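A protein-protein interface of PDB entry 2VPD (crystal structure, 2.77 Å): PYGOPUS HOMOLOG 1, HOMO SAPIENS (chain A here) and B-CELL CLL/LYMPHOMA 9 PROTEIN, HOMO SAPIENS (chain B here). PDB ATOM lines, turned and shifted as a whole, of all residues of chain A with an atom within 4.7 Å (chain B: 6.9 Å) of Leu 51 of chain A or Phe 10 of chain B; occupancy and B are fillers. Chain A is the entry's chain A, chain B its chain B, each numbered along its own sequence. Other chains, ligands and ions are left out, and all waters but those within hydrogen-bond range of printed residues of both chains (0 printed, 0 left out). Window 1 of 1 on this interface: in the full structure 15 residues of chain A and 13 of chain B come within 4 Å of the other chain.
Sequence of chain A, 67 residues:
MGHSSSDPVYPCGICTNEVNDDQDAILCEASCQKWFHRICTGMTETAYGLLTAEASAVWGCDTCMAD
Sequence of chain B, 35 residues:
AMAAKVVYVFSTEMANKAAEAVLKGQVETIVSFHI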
ATOM      1  N   ILE A  26     -10.620 -10.188  11.311  1.00  0.00           N
ATOM      2  CA  ILE A  26     -11.698  -9.357  10.806  1.00  0.00           C
ATOM      3  C   ILE A  26     -13.014  -9.700  11.505  1.00  0.00           C
ATOM      4  O   ILE A  26     -13.275 -10.860  11.850  1.00  0.00           O
ATOM      5  CB  ILE A  26     -11.801  -9.442   9.248  1.00  0.00           C
ATOM      6  CG1 ILE A  26     -12.647  -8.298   8.687  1.00  0.00           C
ATOM      7  CG2 ILE A  26     -12.323 -10.791   8.803  1.00  0.00           C
ATOM      8  CD1 ILE A  26     -12.314  -7.931   7.265  1.00  0.00           C
ATOM      9  N   MET A  43     -10.028 -14.304   2.388  1.00  0.00           N
ATOM     10  CA  MET A  43      -9.831 -12.926   1.967  1.00  0.00           C
ATOM     11  C   MET A  43      -8.348 -12.633   1.760  1.00  0.00           C
ATOM     12  O   MET A  43      -7.524 -12.908   2.628  1.00  0.00           O
ATOM     13  CB  MET A  43     -10.440 -11.968   2.992  1.00  0.00           C
ATOM     14  CG  MET A  43     -10.152 -10.510   2.741  1.00  0.00           C
ATOM     15  SD  MET A  43     -10.931  -9.448   3.966  1.00  0.00           S
ATOM     16  CE  MET A  43     -12.647  -9.548   3.470  1.00  0.00           C
ATOM     17  N   ALA A  47      -7.517  -7.306  -0.243  1.00  0.00           N
ATOM     18  CA  ALA A  47      -8.912  -7.055   0.109  1.00  0.00           C
ATOM     19  C   ALA A  47      -9.021  -6.552   1.551  1.00  0.00           C
ATOM     20  O   ALA A  47      -9.689  -5.554   1.815  1.00  0.00           O
ATOM     21  CB  ALA A  47      -9.743  -8.303  -0.101  1.00  0.00           C
ATOM     22  N   TYR A  48      -8.336  -7.238   2.465  1.00  0.00           N
ATOM     23  CA  TYR A  48      -8.197  -6.802   3.843  1.00  0.00           C
ATOM     24  C   TYR A  48      -7.725  -5.348   3.937  1.00  0.00           C
ATOM     25  O   TYR A  48      -8.406  -4.497   4.510  1.00  0.00           O
ATOM     26  CB  TYR A  48      -7.204  -7.699   4.561  1.00  0.00           C
ATOM     27  CG  TYR A  48      -7.135  -7.423   6.029  1.00  0.00           C
ATOM     28  CD1 TYR A  48      -8.080  -7.970   6.895  1.00  0.00           C
ATOM     29  CD2 TYR A  48      -6.143  -6.591   6.562  1.00  0.00           C
ATOM     30  CE1 TYR A  48      -8.038  -7.709   8.256  1.00  0.00           C
ATOM     31  CE2 TYR A  48      -6.093  -6.321   7.925  1.00  0.00           C
ATOM     32  CZ  TYR A  48      -7.047  -6.889   8.761  1.00  0.00           C
ATOM     33  OH  TYR A  48      -7.023  -6.638  10.111  1.00  0.00           O
ATOM     34  N   GLY A  49      -6.553  -5.076   3.366  1.00  0.00           N
ATOM     35  CA  GLY A  49      -5.998  -3.733   3.337  1.00  0.00           C
ATOM     36  C   GLY A  49      -7.032  -2.707   2.922  1.00  0.00           C
ATOM     37  O   GLY A  49      -7.304  -1.756   3.657  1.00  0.00           O
ATOM     38  N   LEU A  50      -7.622  -2.915   1.750  1.00  0.00           N
ATOM     39  CA  LEU A  50      -8.545  -1.956   1.163  1.00  0.00           C
ATOM     40  C   LEU A  50      -9.833  -1.781   1.966  1.00  0.00           C
ATOM     41  O   LEU A  50     -10.286  -0.653   2.190  1.00  0.00           O
ATOM     42  CB  LEU A  50      -8.867  -2.346  -0.284  1.00  0.00           C
ATOM     43  CG  LEU A  50      -7.780  -2.115  -1.339  1.00  0.00           C
ATOM     44  CD1 LEU A  50      -8.259  -2.556  -2.724  1.00  0.00           C
ATOM     45  CD2 LEU A  50      -7.324  -0.656  -1.372  1.00  0.00           C
ATOM     46  N   LEU A  51     -10.406  -2.898   2.401  1.00  0.00           N
ATOM     47  CA  LEU A  51     -11.669  -2.899   3.130  1.00  0.00           C
ATOM     48  C   LEU A  51     -11.558  -2.177   4.478  1.00  0.00           C
ATOM     49  O   LEU A  51     -12.453  -1.428   4.862  1.00  0.00           O
ATOM     50  CB  LEU A  51     -12.145  -4.343   3.329  1.00  0.00           C
ATOM     51  CG  LEU A  51     -13.629  -4.655   3.509  1.00  0.00           C
ATOM     52  CD1 LEU A  51     -14.375  -4.492   2.212  1.00  0.00           C
ATOM     53  CD2 LEU A  51     -13.770  -6.073   3.990  1.00  0.00           C
ATOM     54  N   THR A  52     -10.456  -2.406   5.188  1.00  0.00           N
ATOM     55  CA  THR A  52     -10.225  -1.772   6.489  1.00  0.00           C
ATOM     56  C   THR A  52      -9.854  -0.289   6.344  1.00  0.00           C
ATOM     57  O   THR A  52     -10.139   0.520   7.227  1.00  0.00           O
ATOM     58  CB  THR A  52      -9.152  -2.511   7.296  1.00  0.00           C
ATOM     59  OG1 THR A  52      -8.019  -2.765   6.461  1.00  0.00           O
ATOM     60  CG2 THR A  52      -9.690  -3.830   7.801  1.00  0.00           C
ATOM     61  N   ALA A  53      -9.238   0.065   5.219  1.00  0.00           N
ATOM     62  CA  ALA A  53      -8.945   1.459   4.914  1.00  0.00           C
ATOM     63  C   ALA A  53     -10.206   2.211   4.494  1.00  0.00           C
ATOM     64  O   ALA A  53     -10.275   3.426   4.644  1.00  0.00           O
ATOM     65  CB  ALA A  53      -7.890   1.555   3.830  1.00  0.00           C
ATOM     66  N   GLU A  54     -11.205   1.494   3.979  1.00  0.00           N
ATOM     67  CA  GLU A  54     -12.417   2.133   3.430  1.00  0.00           C
ATOM     68  C   GLU A  54     -13.469   2.483   4.489  1.00  0.00           C
ATOM     69  O   GLU A  54     -14.009   1.608   5.175  1.00  0.00           O
ATOM     70  CB  GLU A  54     -13.013   1.290   2.296  1.00  0.00           C
ATOM     71  CG  GLU A  54     -14.343   1.792   1.758  1.00  0.00           C
ATOM     72  CD  GLU A  54     -14.275   3.194   1.175  1.00  0.00           C
ATOM     73  OE1 GLU A  54     -13.409   3.437   0.298  1.00  0.00           O
ATOM     74  OE2 GLU A  54     -15.105   4.043   1.582  1.00  0.00           O
ATOM     75  N   ALA A  57     -17.343   0.956   4.315  1.00  0.00           N
ATOM     76  CA  ALA A  57     -17.465  -0.461   4.009  1.00  0.00           C
ATOM     77  C   ALA A  57     -17.380  -1.257   5.293  1.00  0.00           C
ATOM     78  O   ALA A  57     -16.721  -0.839   6.242  1.00  0.00           O
ATOM     79  CB  ALA A  57     -16.371  -0.897   3.047  1.00  0.00           C
ATOM     80  N   VAL A  58     -18.074  -2.384   5.332  1.00  0.00           N
ATOM     81  CA  VAL A  58     -17.907  -3.352   6.405  1.00  0.00           C
ATOM     82  C   VAL A  58     -17.921  -4.729   5.782  1.00  0.00           C
ATOM     83  O   VAL A  58     -18.307  -4.886   4.631  1.00  0.00           O
ATOM     84  CB  VAL A  58     -19.000  -3.255   7.517  1.00  0.00           C
ATOM     85  CG1 VAL A  58     -18.808  -2.003   8.377  1.00  0.00           C
ATOM     86  CG2 VAL A  58     -20.405  -3.328   6.937  1.00  0.00           C
ATOM     87  N   TRP A  59     -17.496  -5.724   6.545  1.00  0.00           N
ATOM     88  CA  TRP A  59     -17.447  -7.090   6.052  1.00  0.00           C
ATOM     89  C   TRP A  59     -18.556  -7.954   6.643  1.00  0.00           C
ATOM     90  O   TRP A  59     -18.986  -7.744   7.777  1.00  0.00           O
ATOM     91  CB  TRP A  59     -16.087  -7.710   6.368  1.00  0.00           C
ATOM     92  CG  TRP A  59     -15.992  -9.149   5.967  1.00  0.00           C
ATOM     93  CD1 TRP A  59     -15.963  -9.649   4.692  1.00  0.00           C
ATOM     94  CD2 TRP A  59     -15.930 -10.279   6.841  1.00  0.00           C
ATOM     95  NE1 TRP A  59     -15.885 -11.013   4.722  1.00  0.00           N
ATOM     96  CE2 TRP A  59     -15.865 -11.429   6.028  1.00  0.00           C
ATOM     97  CE3 TRP A  59     -15.922 -10.431   8.232  1.00  0.00           C
ATOM     98  CZ2 TRP A  59     -15.792 -12.713   6.561  1.00  0.00           C
ATOM     99  CZ3 TRP A  59     -15.852 -11.709   8.758  1.00  0.00           C
ATOM    100  CH2 TRP A  59     -15.782 -12.831   7.924  1.00  0.00           C
ATOM    101  N   GLY A  60     -19.008  -8.934   5.870  1.00  0.00           N
ATOM    102  CA  GLY A  60     -19.941  -9.937   6.372  1.00  0.00           C
ATOM    103  C   GLY A  60     -19.526 -11.352   6.020  1.00  0.00           C
ATOM    104  O   GLY A  60     -19.236 -11.651   4.857  1.00  0.00           O
ATOM    105  N   MET A  65     -24.268 -13.600   5.071  1.00  0.00           N
ATOM    106  CA  MET A  65     -24.668 -13.026   3.776  1.00  0.00           C
ATOM    107  C   MET A  65     -25.730 -13.858   3.050  1.00  0.00           C
ATOM    108  O   MET A  65     -26.542 -13.310   2.299  1.00  0.00           O
ATOM    109  CB  MET A  65     -23.455 -12.830   2.855  1.00  0.00           C
ATOM    110  CG  MET A  65     -22.387 -11.868   3.376  1.00  0.00           C
ATOM    111  SD  MET A  65     -22.973 -10.192   3.648  1.00  0.00           S
ATOM    112  CE  MET A  65     -23.036  -9.535   1.993  1.00  0.00           C
ATOM    113  N   TYR B   8     -21.950  -0.097   3.022  1.00  0.00           N
ATOM    114  CA  TYR B   8     -21.952  -1.232   2.113  1.00  0.00           C
ATOM    115  C   TYR B   8     -21.267  -2.425   2.763  1.00  0.00           C
ATOM    116  O   TYR B   8     -20.134  -2.323   3.239  1.00  0.00           O
ATOM    117  CB  TYR B   8     -21.265  -0.849   0.804  1.00  0.00           C
ATOM    118  CG  TYR B   8     -21.897   0.359   0.178  1.00  0.00           C
ATOM    119  CD1 TYR B   8     -23.069   0.243  -0.563  1.00  0.00           C
ATOM    120  CD2 TYR B   8     -21.344   1.628   0.353  1.00  0.00           C
ATOM    121  CE1 TYR B   8     -23.673   1.351  -1.131  1.00  0.00           C
ATOM    122  CE2 TYR B   8     -21.933   2.750  -0.216  1.00  0.00           C
ATOM    123  CZ  TYR B   8     -23.102   2.604  -0.958  1.00  0.00           C
ATOM    124  OH  TYR B   8     -23.709   3.708  -1.524  1.00  0.00           O
ATOM    125  N   VAL B   9     -21.973  -3.547   2.792  1.00  0.00           N
ATOM    126  CA  VAL B   9     -21.452  -4.783   3.368  1.00  0.00           C
ATOM    127  C   VAL B   9     -20.862  -5.652   2.256  1.00  0.00           C
ATOM    128  O   VAL B   9     -21.522  -5.898   1.245  1.00  0.00           O
ATOM    129  CB  VAL B   9     -22.571  -5.568   4.098  1.00  0.00           C
ATOM    130  CG1 VAL B   9     -21.999  -6.768   4.824  1.00  0.00           C
ATOM    131  CG2 VAL B   9     -23.330  -4.663   5.070  1.00  0.00           C
ATOM    132  N   PHE B  10     -19.625  -6.104   2.433  1.00  0.00           N
ATOM    133  CA  PHE B  10     -18.974  -6.939   1.436  1.00  0.00           C
ATOM    134  C   PHE B  10     -18.862  -8.364   1.921  1.00  0.00           C
ATOM    135  O   PHE B  10     -18.483  -8.602   3.070  1.00  0.00           O
ATOM    136  CB  PHE B  10     -17.564  -6.443   1.166  1.00  0.00           C
ATOM    137  CG  PHE B  10     -17.496  -5.180   0.380  1.00  0.00           C
ATOM    138  CD1 PHE B  10     -17.019  -5.191  -0.922  1.00  0.00           C
ATOM    139  CD2 PHE B  10     -17.865  -3.963   0.947  1.00  0.00           C
ATOM    140  CE1 PHE B  10     -16.932  -4.011  -1.664  1.00  0.00           C
ATOM    141  CE2 PHE B  10     -17.781  -2.773   0.210  1.00  0.00           C
ATOM    142  CZ  PHE B  10     -17.311  -2.801  -1.096  1.00  0.00           C
ATOM    143  N   SER B  11     -19.173  -9.312   1.043  1.00  0.00           N
ATOM    144  CA  SER B  11     -18.815 -10.711   1.265  1.00  0.00           C
ATOM    145  C   SER B  11     -17.333 -10.849   0.973  1.00  0.00           C
ATOM    146  O   SER B  11     -16.726  -9.937   0.414  1.00  0.00           O
ATOM    147  CB  SER B  11     -19.597 -11.622   0.325  1.00  0.00           C
ATOM    148  OG  SER B  11     -19.433 -11.219  -1.030  1.00  0.00           O
ATOM    149  N   THR B  12     -16.746 -11.985   1.326  1.00  0.00           N
ATOM    150  CA  THR B  12     -15.351 -12.225   0.991  1.00  0.00           C
ATOM    151  C   THR B  12     -15.137 -12.226  -0.534  1.00  0.00           C
ATOM    152  O   THR B  12     -14.138 -11.694  -1.031  1.00  0.00           O
ATOM    153  CB  THR B  12     -14.852 -13.518   1.632  1.00  0.00           C
ATOM    154  OG1 THR B  12     -14.911 -13.387   3.058  1.00  0.00           O
ATOM    155  CG2 THR B  12     -13.424 -13.808   1.227  1.00  0.00           C
ATOM    156  N   GLU B  13     -16.089 -12.807  -1.267  1.00  0.00           N
ATOM    157  CA  GLU B  13     -16.010 -12.886  -2.728  1.00  0.00           C
ATOM    158  C   GLU B  13     -16.023 -11.493  -3.326  1.00  0.00           C
ATOM    159  O   GLU B  13     -15.151 -11.135  -4.121  1.00  0.00           O
ATOM    160  CB  GLU B  13     -17.165 -13.714  -3.286  1.00  0.00           C
ATOM    161  CG  GLU B  13     -17.226 -13.788  -4.808  1.00  0.00           C
ATOM    162  CD  GLU B  13     -17.852 -15.098  -5.320  1.00  0.00           C
ATOM    163  OE1 GLU B  13     -18.834 -15.596  -4.706  1.00  0.00           O
ATOM    164  OE2 GLU B  13     -17.354 -15.631  -6.345  1.00  0.00           O
ATOM    165  N   MET B  14     -17.018 -10.712  -2.917  1.00  0.00           N
ATOM    166  CA  MET B  14     -17.172  -9.336  -3.360  1.00  0.00           C
ATOM    167  C   MET B  14     -15.924  -8.507  -3.044  1.00  0.00           C
ATOM    168  O   MET B  14     -15.508  -7.681  -3.857  1.00  0.00           O
ATOM    169  CB  MET B  14     -18.414  -8.716  -2.713  1.00  0.00           C
ATOM    170  CG  MET B  14     -18.897  -7.411  -3.348  1.00  0.00           C
ATOM    171  SD  MET B  14     -19.158  -7.530  -5.138  1.00  0.00           S
ATOM    172  CE  MET B  14     -20.121  -6.049  -5.454  1.00  0.00           C
ATOM    173  N   ALA B  15     -15.328  -8.749  -1.876  1.00  0.00           N
ATOM    174  CA  ALA B  15     -14.133  -8.021  -1.444  1.00  0.00           C
ATOM    175  C   ALA B  15     -12.941  -8.367  -2.322  1.00  0.00           C
ATOM    176  O   ALA B  15     -12.278  -7.475  -2.855  1.00  0.00           O
ATOM    177  CB  ALA B  15     -13.826  -8.310   0.014  1.00  0.00           C
ATOM    178  N   ASN B  16     -12.686  -9.665  -2.486  1.00  0.00           N
ATOM    179  CA  ASN B  16     -11.622 -10.133  -3.361  1.00  0.00           C
ATOM    180  C   ASN B  16     -11.779  -9.630  -4.794  1.00  0.00           C
ATOM    181  O   ASN B  16     -10.792  -9.285  -5.439  1.00  0.00           O
ATOM    182  CB  ASN B  16     -11.526 -11.655  -3.328  1.00  0.00           C
ATOM    183  CG  ASN B  16     -10.899 -12.173  -2.048  1.00  0.00           C
ATOM    184  OD1 ASN B  16     -10.309 -11.423  -1.269  1.00  0.00           O
ATOM    185  ND2 ASN B  16     -11.023 -13.470  -1.825  1.00  0.00           N
ATOM    186  N   ALA B  18     -13.495  -6.825  -5.724  1.00  0.00           N
ATOM    187  CA  ALA B  18     -13.322  -5.383  -5.714  1.00  0.00           C
ATOM    188  C   ALA B  18     -11.840  -5.019  -5.631  1.00  0.00           C
ATOM    189  O   ALA B  18     -11.400  -4.036  -6.237  1.00  0.00           O
ATOM    190  CB  ALA B  18     -14.094  -4.771  -4.575  1.00  0.00           C
ATOM    191  N   ILE B  30     -12.988   0.464  -3.768  1.00  0.00           N
ATOM    192  CA  ILE B  30     -13.773  -0.768  -3.668  1.00  0.00           C
ATOM    193  C   ILE B  30     -15.269  -0.501  -3.539  1.00  0.00           C
ATOM    194  O   ILE B  30     -16.078  -1.409  -3.741  1.00  0.00           O
ATOM    195  CB  ILE B  30     -13.312  -1.656  -2.492  1.00  0.00           C
ATOM    196  CG1 ILE B  30     -13.316  -0.859  -1.182  1.00  0.00           C
ATOM    197  CG2 ILE B  30     -11.937  -2.249  -2.783  1.00  0.00           C
ATOM    198  CD1 ILE B  30     -13.471  -1.704   0.047  1.00  0.00           C
ATOM    199  N   VAL B  31     -15.624   0.737  -3.195  1.00  0.00           N
ATOM    200  CA  VAL B  31     -17.026   1.151  -3.111  1.00  0.00           C
ATOM    201  C   VAL B  31     -17.479   1.905  -4.360  1.00  0.00           C
ATOM    202  O   VAL B  31     -18.598   2.419  -4.412  1.00  0.00           O
ATOM    203  CB  VAL B  31     -17.331   1.999  -1.844  1.00  0.00           C
ATOM    204  CG1 VAL B  31     -17.448   1.110  -0.621  1.00  0.00           C
ATOM    205  CG2 VAL B  31     -16.290   3.096  -1.644  1.00  0.00           C
ATOM    206  N   SER B  32     -16.603   1.958  -5.363  1.00  0.00           N
ATOM    207  CA  SER B  32     -16.888   2.632  -6.630  1.00  0.00           C
ATOM    208  C   SER B  32     -17.791   1.775  -7.517  1.00  0.00           C
ATOM    209  O   SER B  32     -17.411   1.370  -8.623  1.00  0.00           O
ATOM    210  CB  SER B  32     -15.582   2.965  -7.356  1.00  0.00           C
ATOM    211  OG  SER B  32     -14.675   3.617  -6.486  1.00  0.00           O
ATOM    212  N   PHE B  33     -18.993   1.501  -7.021  1.00  0.00           N
ATOM    213  CA  PHE B  33     -19.943   0.657  -7.737  1.00  0.00           C
ATOM    214  C   PHE B  33     -20.474   1.355  -8.975  1.00  0.00           C
ATOM    215  O   PHE B  33     -20.842   2.534  -8.946  1.00  0.00           O
ATOM    216  CB  PHE B  33     -21.105   0.229  -6.836  1.00  0.00           C
ATOM    217  CG  PHE B  33     -20.677  -0.503  -5.600  1.00  0.00           C
ATOM    218  CD1 PHE B  33     -20.256  -1.830  -5.670  1.00  0.00           C
ATOM    219  CD2 PHE B  33     -20.700   0.132  -4.362  1.00  0.00           C
ATOM    220  CE1 PHE B  33     -19.856  -2.512  -4.521  1.00  0.00           C
ATOM    221  CE2 PHE B  33     -20.302  -0.540  -3.212  1.00  0.00           C
ATOM    222  CZ  PHE B  33     -19.881  -1.865  -3.290  1.00  0.00           C
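Leu 51 of chain A touches just these residues of chain B: Phe 10 and Ile 30. Phe 10 of chain B touches five residues of chain A. Printed residues of chain B within 4 Å of Glu 54 of chain A: Ile 30 and Val 31. Printed residues of chain A within 4 Å of Tyr 8 of chain B: Ala 57 and Val 58. The nearest printed residue of chain B that does not touch Met 65 of chain A is Phe 10 of chain B (4.3 Å).
The backbone NH of Gly 60 of chain A lies within hydrogen-bond range of the backbone carbonyl oxygen of Phe 10 of chain B, at 2.9 Å. OG1 of Thr 12 of chain B is in hydrogen-bond range of NE1 of Trp 59 of chain A. O of Tyr 8 of chain B sits at hydrogen-bond distance from N of Val 58 of chain A (2.9 Å). The backbone carbonyl oxygen (O) of Val 58 of chain A is in hydrogen-bond range of the backbone NH (N) of Phe 10 of chain B.
OG of Ser 11 of chain B is in hydrogen-bond range of N of Met 14 of chain B, 3.1 Å away. The side-chain sulfur (SD) of Met 43 of chain A sits at hydrogen-bond distance from the backbone NH (N) of Tyr 48 of chain A.
Of the 14 printed residues of chain B, 9 touch a printed residue of chain A. Hydrophobic or aromatic side chains of chain B within 4 Å of the printed part of chain A: Val 9, Phe 10, Ala 15, Ile 30 and Val 31. Along chain A the printed residues that touch a printed residue of chain B span positions 43 to 65. Among the printed residues, 22 pairs touch across the chains. Among the printed residues, no Asp or Glu carboxylate lies within 4 Å of a Lys or Arg side-chain nitrogen of the other chain.
Among the printed residues, merely in contact across the chains: Met 43 of chain A with Thr 12 of chain B (3.6 Å), Met 43 of chain A with Ala 15 of chain B (3.9 Å), Met 43 of chain A with Asn 16 of chain B (3.6 Å), Ala 47 of chain A with Ala 15 of chain B (3.8 Å), Ala 47 of chain A with Asn 16 of chain B (3.4 Å), Leu 50 of chain A with Ile 30 of chain B (3.7 Å), Leu 51 of chain A with Phe 10 of chain B (3.7 Å), Leu 51 of chain A with Ile 30 of chain B (3.6 Å), Glu 54 of chain A with Ile 30 of chain B (3.8 Å), Glu 54 of chain A with Val 31 of chain B (3.5 Å), Ala 57 of chain A with Tyr 8 of chain B (3.3 Å), Ala 57 of chain A with Phe 10 of chain B (3.7 Å), Val 58 of chain A with Val 9 of chain B (3.4 Å), Trp 59 of chain A with Phe 10 of chain B (3.2 Å), Gly 60 of chain A with Val 9 of chain B (3.8 Å), Gly 60 of chain A with Ser 11 of chain B (3.7 Å), Met 65 of chain A with Val 9 of chain B (3.7 Å) and Met 65 of chain A with Ser 11 of chain B (3.98 Å).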
